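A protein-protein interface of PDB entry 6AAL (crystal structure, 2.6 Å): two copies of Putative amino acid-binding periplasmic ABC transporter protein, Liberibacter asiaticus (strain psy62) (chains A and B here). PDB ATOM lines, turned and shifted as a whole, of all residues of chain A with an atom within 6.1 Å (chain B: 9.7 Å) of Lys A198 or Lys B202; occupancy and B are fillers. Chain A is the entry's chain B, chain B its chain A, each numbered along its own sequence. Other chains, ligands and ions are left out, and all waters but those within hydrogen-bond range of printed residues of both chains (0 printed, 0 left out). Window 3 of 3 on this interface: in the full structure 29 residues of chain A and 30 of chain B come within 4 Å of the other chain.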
ATOM      1  N   GLN A  83      21.981  21.235 -25.273  1.00  0.00           N
ATOM      2  CA  GLN A  83      22.508  19.879 -25.316  1.00  0.00           C
ATOM      3  C   GLN A  83      21.450  18.834 -24.921  1.00  0.00           C
ATOM      4  O   GLN A  83      21.473  17.748 -25.476  1.00  0.00           O
ATOM      5  CB  GLN A  83      23.799  19.743 -24.498  1.00  0.00           C
ATOM      6  CG  GLN A  83      24.558  18.421 -24.678  1.00  0.00           C
ATOM      7  CD  GLN A  83      25.088  18.176 -26.084  1.00  0.00           C
ATOM      8  OE1 GLN A  83      26.292  18.062 -26.294  1.00  0.00           O
ATOM      9  NE2 GLN A  83      24.191  18.066 -27.045  1.00  0.00           N
ATOM     10  N   LYS A  84      20.525  19.159 -24.010  1.00  0.00           N
ATOM     11  CA  LYS A  84      19.366  18.274 -23.696  1.00  0.00           C
ATOM     12  C   LYS A  84      18.561  17.933 -24.940  1.00  0.00           C
ATOM     13  O   LYS A  84      18.356  16.761 -25.259  1.00  0.00           O
ATOM     14  CB  LYS A  84      18.373  18.930 -22.707  1.00  0.00           C
ATOM     15  CG  LYS A  84      18.785  18.986 -21.231  1.00  0.00           C
ATOM     16  CD  LYS A  84      18.269  17.811 -20.385  1.00  0.00           C
ATOM     17  CE  LYS A  84      18.652  17.934 -18.897  1.00  0.00           C
ATOM     18  NZ  LYS A  84      18.039  16.963 -17.941  1.00  0.00           N
ATOM     19  N   LYS A  85      18.100  18.984 -25.629  1.00  0.00           N
ATOM     20  CA  LYS A  85      17.098  18.866 -26.694  1.00  0.00           C
ATOM     21  C   LYS A  85      17.679  18.696 -28.100  1.00  0.00           C
ATOM     22  O   LYS A  85      16.953  18.320 -28.999  1.00  0.00           O
ATOM     23  CB  LYS A  85      16.188  20.106 -26.707  1.00  0.00           C
ATOM     24  CG  LYS A  85      15.188  20.219 -25.558  1.00  0.00           C
ATOM     25  CD  LYS A  85      14.549  21.621 -25.497  1.00  0.00           C
ATOM     26  CE  LYS A  85      13.572  21.912 -26.662  1.00  0.00           C
ATOM     27  NZ  LYS A  85      13.264  23.359 -26.934  1.00  0.00           N
ATOM     28  N   TYR A  86      18.956  19.020 -28.317  1.00  0.00           N
ATOM     29  CA  TYR A  86      19.531  18.970 -29.653  1.00  0.00           C
ATOM     30  C   TYR A  86      20.865  18.270 -29.661  1.00  0.00           C
ATOM     31  O   TYR A  86      21.434  17.933 -28.609  1.00  0.00           O
ATOM     32  CB  TYR A  86      19.708  20.373 -30.211  1.00  0.00           C
ATOM     33  CG  TYR A  86      18.427  21.159 -30.242  1.00  0.00           C
ATOM     34  CD1 TYR A  86      17.589  21.134 -31.348  1.00  0.00           C
ATOM     35  CD2 TYR A  86      18.034  21.912 -29.148  1.00  0.00           C
ATOM     36  CE1 TYR A  86      16.409  21.857 -31.366  1.00  0.00           C
ATOM     37  CE2 TYR A  86      16.854  22.621 -29.151  1.00  0.00           C
ATOM     38  CZ  TYR A  86      16.036  22.596 -30.254  1.00  0.00           C
ATOM     39  OH  TYR A  86      14.851  23.332 -30.212  1.00  0.00           O
ATOM     40  N   ASP A  87      21.361  18.048 -30.870  1.00  0.00           N
ATOM     41  CA  ASP A  87      22.708  17.589 -31.079  1.00  0.00           C
ATOM     42  C   ASP A  87      23.633  18.759 -31.428  1.00  0.00           C
ATOM     43  O   ASP A  87      23.318  19.582 -32.298  1.00  0.00           O
ATOM     44  CB  ASP A  87      22.723  16.575 -32.223  1.00  0.00           C
ATOM     45  CG  ASP A  87      22.270  15.207 -31.792  1.00  0.00           C
ATOM     46  OD1 ASP A  87      22.093  15.021 -30.583  1.00  0.00           O
ATOM     47  OD2 ASP A  87      22.125  14.322 -32.661  1.00  0.00           O
ATOM     48  N   MET A 196      22.001  20.482 -34.673  1.00  0.00           N
ATOM     49  CA  MET A 196      21.112  19.555 -35.412  1.00  0.00           C
ATOM     50  C   MET A 196      19.966  19.107 -34.501  1.00  0.00           C
ATOM     51  O   MET A 196      20.061  19.186 -33.274  1.00  0.00           O
ATOM     52  CB  MET A 196      21.859  18.295 -35.814  1.00  0.00           C
ATOM     53  CG  MET A 196      22.776  18.416 -37.022  1.00  0.00           C
ATOM     54  SD  MET A 196      24.298  19.311 -36.707  1.00  0.00           S
ATOM     55  CE  MET A 196      25.264  18.219 -35.670  1.00  0.00           C
ATOM     56  N   ARG A 197      18.883  18.603 -35.079  1.00  0.00           N
ATOM     57  CA  ARG A 197      17.851  17.969 -34.259  1.00  0.00           C
ATOM     58  C   ARG A 197      18.472  16.826 -33.463  1.00  0.00           C
ATOM     59  O   ARG A 197      19.484  16.230 -33.870  1.00  0.00           O
ATOM     60  CB  ARG A 197      16.738  17.398 -35.138  1.00  0.00           C
ATOM     61  CG  ARG A 197      15.829  18.406 -35.825  1.00  0.00           C
ATOM     62  CD  ARG A 197      14.803  17.692 -36.714  1.00  0.00           C
ATOM     63  NE  ARG A 197      15.395  17.254 -37.994  1.00  0.00           N
ATOM     64  CZ  ARG A 197      15.717  18.073 -39.002  1.00  0.00           C
ATOM     65  NH1 ARG A 197      15.502  19.399 -38.925  1.00  0.00           N
ATOM     66  NH2 ARG A 197      16.250  17.565 -40.110  1.00  0.00           N
ATOM     67  N   LYS A 198      17.867  16.517 -32.322  1.00  0.00           N
ATOM     68  CA  LYS A 198      18.279  15.350 -31.562  1.00  0.00           C
ATOM     69  C   LYS A 198      18.140  14.100 -32.445  1.00  0.00           C
ATOM     70  O   LYS A 198      17.201  13.992 -33.207  1.00  0.00           O
ATOM     71  CB  LYS A 198      17.431  15.216 -30.292  1.00  0.00           C
ATOM     72  CG  LYS A 198      18.216  14.636 -29.128  1.00  0.00           C
ATOM     73  CD  LYS A 198      17.559  14.901 -27.779  1.00  0.00           C
ATOM     74  CE  LYS A 198      16.560  13.809 -27.428  1.00  0.00           C
ATOM     75  NZ  LYS A 198      15.644  14.174 -26.322  1.00  0.00           N
ATOM     76  N   GLY A 199      19.083  13.169 -32.370  1.00  0.00           N
ATOM     77  CA  GLY A 199      18.989  11.920 -33.158  1.00  0.00           C
ATOM     78  C   GLY A 199      19.850  11.844 -34.410  1.00  0.00           C
ATOM     79  O   GLY A 199      20.313  10.769 -34.797  1.00  0.00           O
ATOM     80  N   ASN A 200      20.058  12.986 -35.053  1.00  0.00           N
ATOM     81  CA  ASN A 200      20.987  13.088 -36.182  1.00  0.00           C
ATOM     82  C   ASN A 200      22.408  12.756 -35.710  1.00  0.00           C
ATOM     83  O   ASN A 200      23.190  13.656 -35.393  1.00  0.00           O
ATOM     84  CB  ASN A 200      20.921  14.499 -36.801  1.00  0.00           C
ATOM     85  CG  ASN A 200      19.697  14.696 -37.693  1.00  0.00           C
ATOM     86  OD1 ASN A 200      19.816  14.848 -38.918  1.00  0.00           O
ATOM     87  ND2 ASN A 200      18.509  14.668 -37.087  1.00  0.00           N
ATOM     88  N   LEU B  47      25.269  12.961 -12.587  1.00  0.00           N
ATOM     89  CA  LEU B  47      24.302  12.040 -13.165  1.00  0.00           C
ATOM     90  C   LEU B  47      23.869  11.007 -12.124  1.00  0.00           C
ATOM     91  O   LEU B  47      23.386   9.932 -12.488  1.00  0.00           O
ATOM     92  CB  LEU B  47      24.927  11.319 -14.355  1.00  0.00           C
ATOM     93  CG  LEU B  47      25.523  12.228 -15.416  1.00  0.00           C
ATOM     94  CD1 LEU B  47      26.400  11.418 -16.358  1.00  0.00           C
ATOM     95  CD2 LEU B  47      24.417  12.945 -16.169  1.00  0.00           C
ATOM     96  N   LEU B  49      25.605   8.811 -10.239  1.00  0.00           N
ATOM     97  CA  LEU B  49      26.190   7.497 -10.426  1.00  0.00           C
ATOM     98  C   LEU B  49      27.374   7.326  -9.513  1.00  0.00           C
ATOM     99  O   LEU B  49      28.175   8.226  -9.350  1.00  0.00           O
ATOM    100  CB  LEU B  49      26.651   7.292 -11.856  1.00  0.00           C
ATOM    101  CG  LEU B  49      25.599   7.420 -12.946  1.00  0.00           C
ATOM    102  CD1 LEU B  49      26.280   7.405 -14.302  1.00  0.00           C
ATOM    103  CD2 LEU B  49      24.573   6.317 -12.851  1.00  0.00           C
ATOM    104  N   ASP B  87      32.115   6.958 -30.090  1.00  0.00           N
ATOM    105  CA  ASP B  87      31.513   8.216 -29.685  1.00  0.00           C
ATOM    106  C   ASP B  87      32.513   8.965 -28.826  1.00  0.00           C
ATOM    107  O   ASP B  87      33.155   8.383 -27.962  1.00  0.00           O
ATOM    108  CB  ASP B  87      30.227   7.987 -28.869  1.00  0.00           C
ATOM    109  CG  ASP B  87      28.961   7.857 -29.739  1.00  0.00           C
ATOM    110  OD1 ASP B  87      29.063   7.787 -30.997  1.00  0.00           O
ATOM    111  OD2 ASP B  87      27.854   7.818 -29.130  1.00  0.00           O
ATOM    112  N   MET B 196      33.655   6.604 -25.917  1.00  0.00           N
ATOM    113  CA  MET B 196      32.582   5.683 -25.645  1.00  0.00           C
ATOM    114  C   MET B 196      32.334   4.927 -26.931  1.00  0.00           C
ATOM    115  O   MET B 196      32.728   5.346 -28.018  1.00  0.00           O
ATOM    116  CB  MET B 196      31.302   6.425 -25.268  1.00  0.00           C
ATOM    117  CG  MET B 196      31.155   6.857 -23.815  1.00  0.00           C
ATOM    118  SD  MET B 196      31.853   8.479 -23.406  1.00  0.00           S
ATOM    119  CE  MET B 196      31.052   9.595 -24.566  1.00  0.00           C
ATOM    120  N   ARG B 197      31.664   3.800 -26.798  1.00  0.00           N
ATOM    121  CA  ARG B 197      31.252   3.022 -27.951  1.00  0.00           C
ATOM    122  C   ARG B 197      30.152   3.757 -28.723  1.00  0.00           C
ATOM    123  O   ARG B 197      29.341   4.453 -28.117  1.00  0.00           O
ATOM    124  CB  ARG B 197      30.751   1.675 -27.474  1.00  0.00           C
ATOM    125  CG  ARG B 197      31.811   0.819 -26.807  1.00  0.00           C
ATOM    126  CD  ARG B 197      31.272  -0.584 -26.566  1.00  0.00           C
ATOM    127  NE  ARG B 197      30.222  -0.567 -25.534  1.00  0.00           N
ATOM    128  CZ  ARG B 197      30.430  -0.556 -24.222  1.00  0.00           C
ATOM    129  NH1 ARG B 197      31.662  -0.575 -23.712  1.00  0.00           N
ATOM    130  NH2 ARG B 197      29.382  -0.525 -23.430  1.00  0.00           N
ATOM    131  N   LYS B 198      30.162   3.639 -30.054  1.00  0.00           N
ATOM    132  CA  LYS B 198      29.140   4.251 -30.911  1.00  0.00           C
ATOM    133  C   LYS B 198      27.772   3.834 -30.438  1.00  0.00           C
ATOM    134  O   LYS B 198      27.606   2.693 -30.021  1.00  0.00           O
ATOM    135  CB  LYS B 198      29.264   3.792 -32.365  1.00  0.00           C
ATOM    136  CG  LYS B 198      30.388   4.429 -33.165  1.00  0.00           C
ATOM    137  CD  LYS B 198      29.907   5.115 -34.466  1.00  0.00           C
ATOM    138  CE  LYS B 198      29.164   4.205 -35.441  1.00  0.00           C
ATOM    139  NZ  LYS B 198      29.796   2.860 -35.527  1.00  0.00           N
ATOM    140  N   GLY B 199      26.797   4.741 -30.523  1.00  0.00           N
ATOM    141  CA  GLY B 199      25.428   4.451 -30.079  1.00  0.00           C
ATOM    142  C   GLY B 199      25.125   4.671 -28.592  1.00  0.00           C
ATOM    143  O   GLY B 199      23.981   4.490 -28.178  1.00  0.00           O
ATOM    144  N   ASN B 200      26.128   5.059 -27.790  1.00  0.00           N
ATOM    145  CA  ASN B 200      25.893   5.532 -26.431  1.00  0.00           C
ATOM    146  C   ASN B 200      25.533   7.025 -26.458  1.00  0.00           C
ATOM    147  O   ASN B 200      26.197   7.879 -25.851  1.00  0.00           O
ATOM    148  CB  ASN B 200      27.114   5.288 -25.546  1.00  0.00           C
ATOM    149  CG  ASN B 200      27.261   3.840 -25.147  1.00  0.00           C
ATOM    150  OD1 ASN B 200      26.889   3.443 -24.038  1.00  0.00           O
ATOM    151  ND2 ASN B 200      27.793   3.034 -26.059  1.00  0.00           N
ATOM    152  N   ASN B 201      24.445   7.326 -27.150  1.00  0.00           N
ATOM    153  CA  ASN B 201      24.130   8.687 -27.484  1.00  0.00           C
ATOM    154  C   ASN B 201      23.518   9.417 -26.331  1.00  0.00           C
ATOM    155  O   ASN B 201      23.817  10.586 -26.142  1.00  0.00           O
ATOM    156  CB  ASN B 201      23.223   8.730 -28.700  1.00  0.00           C
ATOM    157  CG  ASN B 201      23.873   8.093 -29.899  1.00  0.00           C
ATOM    158  OD1 ASN B 201      23.542   6.974 -30.233  1.00  0.00           O
ATOM    159  ND2 ASN B 201      24.859   8.771 -30.500  1.00  0.00           N
ATOM    160  N   LYS B 202      22.682   8.772 -25.539  1.00  0.00           N
ATOM    161  CA  LYS B 202      22.101   9.521 -24.438  1.00  0.00           C
ATOM    162  C   LYS B 202      23.161   9.786 -23.394  1.00  0.00           C
ATOM    163  O   LYS B 202      23.180  10.854 -22.762  1.00  0.00           O
ATOM    164  CB  LYS B 202      20.882   8.836 -23.808  1.00  0.00           C
ATOM    165  CG  LYS B 202      20.015   9.760 -22.919  1.00  0.00           C
ATOM    166  CD  LYS B 202      19.783  11.211 -23.431  1.00  0.00           C
ATOM    167  CE  LYS B 202      18.948  11.319 -24.724  1.00  0.00           C
ATOM    168  NZ  LYS B 202      17.466  11.370 -24.547  1.00  0.00           N
ATOM    169  N   LEU B 203      24.052   8.821 -23.214  1.00  0.00           N
ATOM    170  CA  LEU B 203      25.157   9.023 -22.287  1.00  0.00           C
ATOM    171  C   LEU B 203      25.973  10.221 -22.741  1.00  0.00           C
ATOM    172  O   LEU B 203      26.211  11.128 -21.968  1.00  0.00           O
ATOM    173  CB  LEU B 203      26.050   7.790 -22.175  1.00  0.00           C
ATOM    174  CG  LEU B 203      27.184   7.924 -21.136  1.00  0.00           C
ATOM    175  CD1 LEU B 203      26.653   8.242 -19.739  1.00  0.00           C
ATOM    176  CD2 LEU B 203      28.075   6.678 -21.098  1.00  0.00           C
ATOM    177  N   THR B 204      26.368  10.237 -24.008  1.00  0.00           N
ATOM    178  CA  THR B 204      27.219  11.296 -24.503  1.00  0.00           C
ATOM    179  C   THR B 204      26.526  12.655 -24.277  1.00  0.00           C
ATOM    180  O   THR B 204      27.157  13.593 -23.758  1.00  0.00           O
ATOM    181  CB  THR B 204      27.623  11.074 -25.976  1.00  0.00           C
ATOM    182  OG1 THR B 204      28.176   9.752 -26.167  1.00  0.00           O
ATOM    183  CG2 THR B 204      28.654  12.105 -26.387  1.00  0.00           C
ATOM    184  N   ARG B 205      25.224  12.740 -24.593  1.00  0.00           N
ATOM    185  CA  ARG B 205      24.449  13.987 -24.383  1.00  0.00           C
ATOM    186  C   ARG B 205      24.444  14.404 -22.933  1.00  0.00           C
ATOM    187  O   ARG B 205      24.406  15.569 -22.625  1.00  0.00           O
ATOM    188  CB  ARG B 205      22.999  13.889 -24.906  1.00  0.00           C
ATOM    189  CG  ARG B 205      22.882  14.055 -26.428  1.00  0.00           C
ATOM    190  CD  ARG B 205      21.451  14.169 -26.962  1.00  0.00           C
ATOM    191  NE  ARG B 205      20.940  12.878 -27.419  1.00  0.00           N
ATOM    192  CZ  ARG B 205      21.197  12.324 -28.607  1.00  0.00           C
ATOM    193  NH1 ARG B 205      21.970  12.918 -29.506  1.00  0.00           N
ATOM    194  NH2 ARG B 205      20.675  11.137 -28.901  1.00  0.00           N
ATOM    195  N   SER B 206      24.521  13.436 -22.043  1.00  0.00           N
ATOM    196  CA  SER B 206      24.457  13.688 -20.618  1.00  0.00           C
ATOM    197  C   SER B 206      25.792  14.154 -20.122  1.00  0.00           C
ATOM    198  O   SER B 206      25.866  15.098 -19.342  1.00  0.00           O
ATOM    199  CB  SER B 206      24.076  12.412 -19.870  1.00  0.00           C
ATOM    200  OG  SER B 206      22.705  12.106 -20.016  1.00  0.00           O
ATOM    201  N   ILE B 207      26.857  13.486 -20.550  1.00  0.00           N
ATOM    202  CA  ILE B 207      28.182  13.895 -20.142  1.00  0.00           C
ATOM    203  C   ILE B 207      28.427  15.308 -20.635  1.00  0.00           C
ATOM    204  O   ILE B 207      28.835  16.159 -19.844  1.00  0.00           O
ATOM    205  CB  ILE B 207      29.284  12.938 -20.657  1.00  0.00           C
ATOM    206  CG1 ILE B 207      29.253  11.604 -19.888  1.00  0.00           C
ATOM    207  CG2 ILE B 207      30.664  13.550 -20.461  1.00  0.00           C
ATOM    208  CD1 ILE B 207      29.902  10.451 -20.631  1.00  0.00           C
ATOM    209  N   ASN B 208      28.169  15.545 -21.926  1.00  0.00           N
ATOM    210  CA  ASN B 208      28.360  16.852 -22.544  1.00  0.00           C
ATOM    211  C   ASN B 208      27.559  17.921 -21.838  1.00  0.00           C
ATOM    212  O   ASN B 208      28.026  19.037 -21.671  1.00  0.00           O
ATOM    213  CB  ASN B 208      27.961  16.841 -24.025  1.00  0.00           C
ATOM    214  CG  ASN B 208      28.902  16.005 -24.902  1.00  0.00           C
ATOM    215  OD1 ASN B 208      29.936  15.483 -24.439  1.00  0.00           O
ATOM    216  ND2 ASN B 208      28.529  15.856 -26.198  1.00  0.00           N
ATOM    217  N   GLU B 209      26.359  17.570 -21.382  1.00  0.00           N
ATOM    218  CA  GLU B 209      25.533  18.531 -20.652  1.00  0.00           C
ATOM    219  C   GLU B 209      26.158  18.859 -19.323  1.00  0.00           C
ATOM    220  O   GLU B 209      26.268  20.031 -18.912  1.00  0.00           O
ATOM    221  CB  GLU B 209      24.137  17.991 -20.425  1.00  0.00           C
ATOM    222  CG  GLU B 209      23.134  19.091 -20.154  1.00  0.00           C
ATOM    223  CD  GLU B 209      21.810  18.579 -19.612  1.00  0.00           C
ATOM    224  OE1 GLU B 209      21.287  19.256 -18.674  1.00  0.00           O
ATOM    225  OE2 GLU B 209      21.306  17.528 -20.132  1.00  0.00           O
ATOM    226  N   ILE B 210      26.564  17.811 -18.632  1.00  0.00           N
ATOM    227  CA  ILE B 210      27.129  17.986 -17.316  1.00  0.00           C
ATOM    228  C   ILE B 210      28.428  18.769 -17.436  1.00  0.00           C
ATOM    229  O   ILE B 210      28.670  19.659 -16.633  1.00  0.00           O
ATOM    230  CB  ILE B 210      27.344  16.643 -16.620  1.00  0.00           C
ATOM    231  CG1 ILE B 210      26.003  15.980 -16.321  1.00  0.00           C
ATOM    232  CG2 ILE B 210      28.125  16.824 -15.342  1.00  0.00           C
ATOM    233  CD1 ILE B 210      25.067  16.773 -15.440  1.00  0.00           C
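The guanidinium group (NH1) of Arg B205 is in salt-bridge range of the side-chain carboxylate (OD2) of Asp A87, at 3.5 Å. The side-chain amino group (NZ) of Lys A84 lies within salt-bridge range of the side-chain carboxylate (OE2) of Glu B209, at 3.97 Å. ND2 of Asn B208 sits close to OE1 of Gln A83.
Positions printed for both chains: 87, 196, 197, 198, 199 and 200. Of the 7 pairs that touch across the chains among the printed residues, none has its exchanged pair printed and touching as well.
O of Arg B205 touches CG of Gln A83, 3.5 Å away. CG of Gln A83 touches N of Glu B209, 3.9 Å away. NZ of Lys B202 touches NZ of Lys A198, at 3.8 Å. Arg B205 touches Lys A198.
Of chain B, only Lys B202 and Arg B205 come within 4 Å of Lys A198. Lys B202 touches just one residue of chain A: Lys A198. No residue of chain B comes within 4 Å of Gly A199. Of the printed residues of chain B, Lys A84 touches Glu B209. Of the printed residues of chain A, Glu B209 touches Gln A83 (3.9 Å) and Lys A84 (3.0 Å). Of the printed residues of chain B, Gln A83 touches Arg B205 (3.5 Å), Asn B208 (3.1 Å) and Glu B209 (3.9 Å). Printed residues of chain A within 4 Å of Asn B208: Gln A83 (3.1 Å). The nearest printed residue of chain A that does not touch Glu B209 is Lys A85 (6.5 Å).
The backbone carbonyl oxygen (O) of Thr B204 sits close to the side-chain amide oxygen (OD1) of Asn B208 (3.4 Å). NE2 of Gln A83 sits at hydrogen-bond distance from O of Tyr A86. The backbone NH (N) of Gly A199 lies within hydrogen-bond range of the side-chain carboxylate (OD2) of Asp A87 (3.3 Å). The side-chain carboxylate of Asp A87 is in hydrogen-bond range of the backbone NH of Asn A200 (3.4 Å). The backbone NH (N) of Met A196 lies within hydrogen-bond range of the backbone carbonyl oxygen (O) of Asp A87, 2.9 Å away. The side-chain hydroxyl of Ser B206 lies within hydrogen-bond range of the backbone carbonyl oxygen of Lys B202, at 3.1 Å.
Of the 10 printed residues of chain A, 4 touch a printed residue of chain B. Printed residues of chain A that touch a printed residue of chain B: Gln A83, Lys A84, Asp A87 and Lys A198. Of the 18 printed residues of chain B, 4 touch a printed residue of chain A. Among the printed residues, 7 pairs touch across the chains.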
